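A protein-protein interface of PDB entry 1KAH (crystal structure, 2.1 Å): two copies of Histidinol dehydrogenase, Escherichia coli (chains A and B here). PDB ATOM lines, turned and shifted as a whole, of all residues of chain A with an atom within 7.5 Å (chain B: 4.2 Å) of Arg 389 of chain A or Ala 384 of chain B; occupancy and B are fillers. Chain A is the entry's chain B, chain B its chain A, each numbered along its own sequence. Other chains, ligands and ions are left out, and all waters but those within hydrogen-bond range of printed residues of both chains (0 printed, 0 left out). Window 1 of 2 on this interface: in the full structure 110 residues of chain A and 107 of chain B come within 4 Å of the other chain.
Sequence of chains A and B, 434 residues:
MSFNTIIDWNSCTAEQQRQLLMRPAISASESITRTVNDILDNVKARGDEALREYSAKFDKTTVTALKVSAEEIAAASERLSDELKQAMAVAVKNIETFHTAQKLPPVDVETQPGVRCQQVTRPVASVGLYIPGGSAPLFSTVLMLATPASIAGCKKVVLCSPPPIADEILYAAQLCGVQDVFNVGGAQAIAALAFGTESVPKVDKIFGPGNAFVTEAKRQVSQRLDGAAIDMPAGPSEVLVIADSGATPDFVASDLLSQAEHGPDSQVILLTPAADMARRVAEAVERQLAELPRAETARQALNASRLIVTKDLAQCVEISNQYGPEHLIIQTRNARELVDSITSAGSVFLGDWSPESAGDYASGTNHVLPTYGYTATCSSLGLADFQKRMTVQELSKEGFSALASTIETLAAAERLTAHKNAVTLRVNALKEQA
N of Gly 382 of chain B is in hydrogen-bond range of OD2 of Asp 385 of chain B, 2.9 Å away. O of Arg 122 of chain A sits at hydrogen-bond distance from N of Lys 388 of chain A (2.7 Å).
Arg 389 of chain A touches five residues of chain B. Of the printed residues of chain B, Thr 391 of chain A touches Ser 380. Printed residues of chain A within 4 Å of Ser 380 of chain B: Arg 389 (3.1 Å) and Thr 391 (3.9 Å). Of the printed residues of chain B, Lys 388 of chain A touches Ser 379. Of the printed residues of chain A, Asp 385 of chain B touches Arg 389. The nearest residue of chain A that does not touch Ala 384 of chain B is Thr 377 of chain A (6.3 Å).
Along chain A the printed residues that touch a printed residue of chain B span positions 388 to 391. Hydrophobic or aromatic side chains of chain B within 4 Å of the printed part of chain A: Ala 384. Among the printed residues, 7 pairs touch across the chains. Among the printed residues, Asp or Glu carboxylates within 4 Å of a Lys or Arg side-chain nitrogen of the other chain: Arg 389 of chain A with Asp 385 of chain B.
Lys 388 of chain A touches Ser 379 of chain B. Gly 382 of chain B touches Arg 389 of chain A (CA to NH1, 3.9 Å). NH2 of Arg 389 of chain A touches CB of Ala 384 of chain B, at 3.7 Å. Ser 380 of chain B touches Thr 391 of chain A (OG to OG1, 3.9 Å).
3 positions are printed for both chains. Of the 7 pairs that touch across the chains among the printed residues, none has its exchanged pair printed and touching as well.
The side-chain hydroxyl (OG) of Ser 379 of chain B lies within hydrogen-bond range of the backbone NH (N) of Arg 389 of chain A, 2.6 Å away. O of Ser 380 of chain B is in hydrogen-bond range of NH1 of Arg 389 of chain A (3.1 Å). NH2 of Arg 389 of chain A lies within salt-bridge range of OD2 of Asp 385 of chain B (3.3 Å).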
ATOM      1  N   LEU A 104     -23.201   0.443 -28.510  1.00  0.00           N
ATOM      2  CA  LEU A 104     -21.803   0.070 -28.282  1.00  0.00           C
ATOM      3  C   LEU A 104     -21.612  -1.014 -27.230  1.00  0.00           C
ATOM      4  O   LEU A 104     -22.242  -0.991 -26.171  1.00  0.00           O
ATOM      5  CB  LEU A 104     -20.972   1.285 -27.854  1.00  0.00           C
ATOM      6  CG  LEU A 104     -20.865   2.511 -28.761  1.00  0.00           C
ATOM      7  CD1 LEU A 104     -19.803   3.441 -28.200  1.00  0.00           C
ATOM      8  CD2 LEU A 104     -20.506   2.099 -30.175  1.00  0.00           C
ATOM      9  N   GLN A 119     -14.891   2.752 -21.030  1.00  0.00           N
ATOM     10  CA  GLN A 119     -15.534   3.741 -21.865  1.00  0.00           C
ATOM     11  C   GLN A 119     -17.008   3.429 -21.703  1.00  0.00           C
ATOM     12  O   GLN A 119     -17.446   2.331 -22.039  1.00  0.00           O
ATOM     13  CB  GLN A 119     -15.161   3.560 -23.331  1.00  0.00           C
ATOM     14  CG  GLN A 119     -15.746   4.623 -24.232  1.00  0.00           C
ATOM     15  CD  GLN A 119     -15.505   4.330 -25.700  1.00  0.00           C
ATOM     16  OE1 GLN A 119     -16.208   3.513 -26.308  1.00  0.00           O
ATOM     17  NE2 GLN A 119     -14.503   4.986 -26.277  1.00  0.00           N
ATOM     18  N   VAL A 120     -17.771   4.371 -21.166  1.00  0.00           N
ATOM     19  CA  VAL A 120     -19.205   4.162 -21.001  1.00  0.00           C
ATOM     20  C   VAL A 120     -19.941   5.268 -21.748  1.00  0.00           C
ATOM     21  O   VAL A 120     -19.372   6.319 -22.046  1.00  0.00           O
ATOM     22  CB  VAL A 120     -19.624   4.182 -19.503  1.00  0.00           C
ATOM     23  CG1 VAL A 120     -18.968   3.018 -18.761  1.00  0.00           C
ATOM     24  CG2 VAL A 120     -19.251   5.507 -18.872  1.00  0.00           C
ATOM     25  N   THR A 121     -21.204   5.032 -22.068  1.00  0.00           N
ATOM     26  CA  THR A 121     -21.961   6.035 -22.780  1.00  0.00           C
ATOM     27  C   THR A 121     -23.004   6.643 -21.876  1.00  0.00           C
ATOM     28  O   THR A 121     -23.479   6.020 -20.925  1.00  0.00           O
ATOM     29  CB  THR A 121     -22.667   5.452 -24.014  1.00  0.00           C
ATOM     30  OG1 THR A 121     -23.599   4.446 -23.599  1.00  0.00           O
ATOM     31  CG2 THR A 121     -21.657   4.848 -24.970  1.00  0.00           C
ATOM     32  N   ARG A 122     -23.331   7.892 -22.160  1.00  0.00           N
ATOM     33  CA  ARG A 122     -24.342   8.599 -21.406  1.00  0.00           C
ATOM     34  C   ARG A 122     -25.110   9.304 -22.501  1.00  0.00           C
ATOM     35  O   ARG A 122     -24.518   9.771 -23.479  1.00  0.00           O
ATOM     36  CB  ARG A 122     -23.704   9.601 -20.436  1.00  0.00           C
ATOM     37  CG  ARG A 122     -22.987   8.963 -19.223  1.00  0.00           C
ATOM     38  CD  ARG A 122     -23.991   8.369 -18.231  1.00  0.00           C
ATOM     39  NE  ARG A 122     -23.356   7.794 -17.045  1.00  0.00           N
ATOM     40  CZ  ARG A 122     -22.753   6.608 -17.008  1.00  0.00           C
ATOM     41  NH1 ARG A 122     -22.696   5.850 -18.095  1.00  0.00           N
ATOM     42  NH2 ARG A 122     -22.207   6.172 -15.881  1.00  0.00           N
ATOM     43  N   PRO A 123     -26.442   9.353 -22.379  1.00  0.00           N
ATOM     44  CA  PRO A 123     -27.261  10.008 -23.391  1.00  0.00           C
ATOM     45  C   PRO A 123     -27.221  11.521 -23.250  1.00  0.00           C
ATOM     46  O   PRO A 123     -26.983  12.041 -22.157  1.00  0.00           O
ATOM     47  CB  PRO A 123     -28.650   9.457 -23.094  1.00  0.00           C
ATOM     48  CG  PRO A 123     -28.636   9.390 -21.601  1.00  0.00           C
ATOM     49  CD  PRO A 123     -27.290   8.759 -21.328  1.00  0.00           C
ATOM     50  N   THR A 377     -15.389  13.537 -43.176  1.00  0.00           N
ATOM     51  CA  THR A 377     -15.128  13.430 -41.746  1.00  0.00           C
ATOM     52  C   THR A 377     -16.342  13.105 -40.882  1.00  0.00           C
ATOM     53  O   THR A 377     -16.189  12.550 -39.798  1.00  0.00           O
ATOM     54  CB  THR A 377     -14.526  14.739 -41.221  1.00  0.00           C
ATOM     55  OG1 THR A 377     -15.357  15.837 -41.641  1.00  0.00           O
ATOM     56  CG2 THR A 377     -13.117  14.933 -41.758  1.00  0.00           C
ATOM     57  N   SER A 379     -20.319  11.402 -40.105  1.00  0.00           N
ATOM     58  CA  SER A 379     -21.010  10.151 -40.383  1.00  0.00           C
ATOM     59  C   SER A 379     -22.508  10.301 -40.520  1.00  0.00           C
ATOM     60  O   SER A 379     -23.076  11.357 -40.258  1.00  0.00           O
ATOM     61  CB  SER A 379     -20.743   9.145 -39.261  1.00  0.00           C
ATOM     62  OG  SER A 379     -19.359   8.970 -39.021  1.00  0.00           O
ATOM     63  N   ALA A 384     -25.018   7.170 -31.939  1.00  0.00           N
ATOM     64  CA  ALA A 384     -23.919   7.907 -31.340  1.00  0.00           C
ATOM     65  C   ALA A 384     -24.148   9.409 -31.233  1.00  0.00           C
ATOM     66  O   ALA A 384     -23.572  10.054 -30.367  1.00  0.00           O
ATOM     67  CB  ALA A 384     -22.627   7.634 -32.114  1.00  0.00           C
ATOM     68  N   GLN A 387     -25.754  10.490 -27.899  1.00  0.00           N
ATOM     69  CA  GLN A 387     -25.007  10.050 -26.718  1.00  0.00           C
ATOM     70  C   GLN A 387     -23.655  10.736 -26.626  1.00  0.00           C
ATOM     71  O   GLN A 387     -23.266  11.512 -27.504  1.00  0.00           O
ATOM     72  CB  GLN A 387     -24.736   8.541 -26.772  1.00  0.00           C
ATOM     73  CG  GLN A 387     -25.865   7.685 -27.289  1.00  0.00           C
ATOM     74  CD  GLN A 387     -25.505   6.215 -27.283  1.00  0.00           C
ATOM     75  OE1 GLN A 387     -24.534   5.798 -27.916  1.00  0.00           O
ATOM     76  NE2 GLN A 387     -26.282   5.421 -26.561  1.00  0.00           N
ATOM     77  N   LYS A 388     -22.939  10.405 -25.553  1.00  0.00           N
ATOM     78  CA  LYS A 388     -21.599  10.923 -25.267  1.00  0.00           C
ATOM     79  C   LYS A 388     -20.773   9.772 -24.681  1.00  0.00           C
ATOM     80  O   LYS A 388     -21.293   8.950 -23.926  1.00  0.00           O
ATOM     81  CB  LYS A 388     -21.662  12.036 -24.218  1.00  0.00           C
ATOM     82  CG  LYS A 388     -22.786  13.031 -24.416  1.00  0.00           C
ATOM     83  CD  LYS A 388     -22.930  13.909 -23.196  1.00  0.00           C
ATOM     84  CE  LYS A 388     -23.341  13.095 -21.977  1.00  0.00           C
ATOM     85  NZ  LYS A 388     -23.229  13.906 -20.740  1.00  0.00           N
ATOM     86  N   ARG A 389     -19.494   9.718 -25.038  1.00  0.00           N
ATOM     87  CA  ARG A 389     -18.585   8.701 -24.527  1.00  0.00           C
ATOM     88  C   ARG A 389     -17.830   9.320 -23.359  1.00  0.00           C
ATOM     89  O   ARG A 389     -17.276  10.412 -23.468  1.00  0.00           O
ATOM     90  CB  ARG A 389     -17.591   8.254 -25.608  1.00  0.00           C
ATOM     91  CG  ARG A 389     -18.194   7.315 -26.666  1.00  0.00           C
ATOM     92  CD  ARG A 389     -17.194   6.964 -27.784  1.00  0.00           C
ATOM     93  NE  ARG A 389     -16.890   8.091 -28.678  1.00  0.00           N
ATOM     94  CZ  ARG A 389     -15.773   8.819 -28.631  1.00  0.00           C
ATOM     95  NH1 ARG A 389     -14.834   8.553 -27.731  1.00  0.00           N
ATOM     96  NH2 ARG A 389     -15.585   9.811 -29.494  1.00  0.00           N
ATOM     97  N   MET A 390     -17.837   8.625 -22.234  1.00  0.00           N
ATOM     98  CA  MET A 390     -17.160   9.094 -21.043  1.00  0.00           C
ATOM     99  C   MET A 390     -16.111   8.055 -20.644  1.00  0.00           C
ATOM    100  O   MET A 390     -16.330   6.847 -20.764  1.00  0.00           O
ATOM    101  CB  MET A 390     -18.190   9.300 -19.931  1.00  0.00           C
ATOM    102  CG  MET A 390     -17.623   9.780 -18.621  1.00  0.00           C
ATOM    103  SD  MET A 390     -19.032  10.356 -17.437  1.00  0.00           S
ATOM    104  CE  MET A 390     -19.692   8.623 -16.875  1.00  0.00           C
ATOM    105  N   THR A 391     -14.959   8.532 -20.196  1.00  0.00           N
ATOM    106  CA  THR A 391     -13.880   7.654 -19.787  1.00  0.00           C
ATOM    107  C   THR A 391     -13.804   7.489 -18.268  1.00  0.00           C
ATOM    108  O   THR A 391     -14.084   8.419 -17.516  1.00  0.00           O
ATOM    109  CB  THR A 391     -12.547   8.180 -20.332  1.00  0.00           C
ATOM    110  OG1 THR A 391     -12.473   7.890 -21.732  1.00  0.00           O
ATOM    111  CG2 THR A 391     -11.394   7.540 -19.641  1.00  0.00           C
ATOM    112  N   SER B 379     -17.620  14.286 -26.536  1.00  0.00           N
ATOM    113  CA  SER B 379     -16.967  13.197 -25.841  1.00  0.00           C
ATOM    114  C   SER B 379     -15.461  13.312 -25.816  1.00  0.00           C
ATOM    115  O   SER B 379     -14.866  14.130 -26.512  1.00  0.00           O
ATOM    116  CB  SER B 379     -17.344  11.868 -26.487  1.00  0.00           C
ATOM    117  OG  SER B 379     -18.748  11.719 -26.549  1.00  0.00           O
ATOM    118  N   SER B 380     -14.852  12.476 -24.988  1.00  0.00           N
ATOM    119  CA  SER B 380     -13.412  12.419 -24.888  1.00  0.00           C
ATOM    120  C   SER B 380     -12.912  12.003 -26.255  1.00  0.00           C
ATOM    121  O   SER B 380     -13.642  11.364 -27.020  1.00  0.00           O
ATOM    122  CB  SER B 380     -12.995  11.351 -23.887  1.00  0.00           C
ATOM    123  OG  SER B 380     -11.687  10.877 -24.191  1.00  0.00           O
ATOM    124  N   GLY B 382     -11.222   9.750 -28.823  1.00  0.00           N
ATOM    125  CA  GLY B 382     -11.121   8.308 -28.844  1.00  0.00           C
ATOM    126  C   GLY B 382     -10.980   7.890 -30.287  1.00  0.00           C
ATOM    127  O   GLY B 382     -10.799   8.731 -31.161  1.00  0.00           O
ATOM    128  N   LEU B 383     -11.068   6.590 -30.536  1.00  0.00           N
ATOM    129  CA  LEU B 383     -10.951   6.044 -31.877  1.00  0.00           C
ATOM    130  C   LEU B 383     -11.956   6.664 -32.845  1.00  0.00           C
ATOM    131  O   LEU B 383     -11.632   6.970 -33.993  1.00  0.00           O
ATOM    132  CB  LEU B 383     -11.179   4.532 -31.823  1.00  0.00           C
ATOM    133  CG  LEU B 383     -10.889   3.748 -33.095  1.00  0.00           C
ATOM    134  CD1 LEU B 383      -9.387   3.820 -33.412  1.00  0.00           C
ATOM    135  CD2 LEU B 383     -11.325   2.298 -32.898  1.00  0.00           C
ATOM    136  N   ALA B 384     -13.180   6.840 -32.367  1.00  0.00           N
ATOM    137  CA  ALA B 384     -14.258   7.377 -33.183  1.00  0.00           C
ATOM    138  C   ALA B 384     -13.953   8.710 -33.860  1.00  0.00           C
ATOM    139  O   ALA B 384     -14.436   8.963 -34.953  1.00  0.00           O
ATOM    140  CB  ALA B 384     -15.530   7.494 -32.341  1.00  0.00           C
ATOM    141  N   ASP B 385     -13.153   9.557 -33.223  1.00  0.00           N
ATOM    142  CA  ASP B 385     -12.832  10.865 -33.796  1.00  0.00           C
ATOM    143  C   ASP B 385     -11.889  10.791 -34.999  1.00  0.00           C
ATOM    144  O   ASP B 385     -11.644  11.804 -35.656  1.00  0.00           O
ATOM    145  CB  ASP B 385     -12.225  11.771 -32.725  1.00  0.00           C
ATOM    146  CG  ASP B 385     -13.171  12.013 -31.570  1.00  0.00           C
ATOM    147  OD1 ASP B 385     -14.209  12.674 -31.782  1.00  0.00           O
ATOM    148  OD2 ASP B 385     -12.886  11.537 -30.448  1.00  0.00           O
ATOM    149  N   PHE B 386     -11.364   9.599 -35.274  1.00  0.00           N
ATOM    150  CA  PHE B 386     -10.455   9.397 -36.406  1.00  0.00           C
ATOM    151  C   PHE B 386     -11.053   8.498 -37.478  1.00  0.00           C
ATOM    152  O   PHE B 386     -10.325   7.928 -38.292  1.00  0.00           O
ATOM    153  CB  PHE B 386      -9.123   8.786 -35.951  1.00  0.00           C
ATOM    154  CG  PHE B 386      -8.326   9.676 -35.055  1.00  0.00           C
ATOM    155  CD1 PHE B 386      -8.643   9.788 -33.702  1.00  0.00           C
ATOM    156  CD2 PHE B 386      -7.275  10.433 -35.567  1.00  0.00           C
ATOM    157  CE1 PHE B 386      -7.922  10.647 -32.871  1.00  0.00           C
ATOM    158  CE2 PHE B 386      -6.552  11.293 -34.748  1.00  0.00           C
ATOM    159  CZ  PHE B 386      -6.877  11.401 -33.397  1.00  0.00           C
ATOM    160  N   GLN B 387     -12.375   8.365 -37.472  1.00  0.00           N
ATOM    161  CA  GLN B 387     -13.043   7.541 -38.458  1.00  0.00           C
ATOM    162  C   GLN B 387     -14.477   8.017 -38.595  1.00  0.00           C
ATOM    163  O   GLN B 387     -14.875   8.983 -37.953  1.00  0.00           O
ATOM    164  CB  GLN B 387     -13.001   6.076 -38.026  1.00  0.00           C
ATOM    165  CG  GLN B 387     -13.849   5.753 -36.819  1.00  0.00           C
ATOM    166  CD  GLN B 387     -13.531   4.386 -36.227  1.00  0.00           C
ATOM    167  OE1 GLN B 387     -14.298   3.851 -35.428  1.00  0.00           O
ATOM    168  NE2 GLN B 387     -12.393   3.823 -36.608  1.00  0.00           N
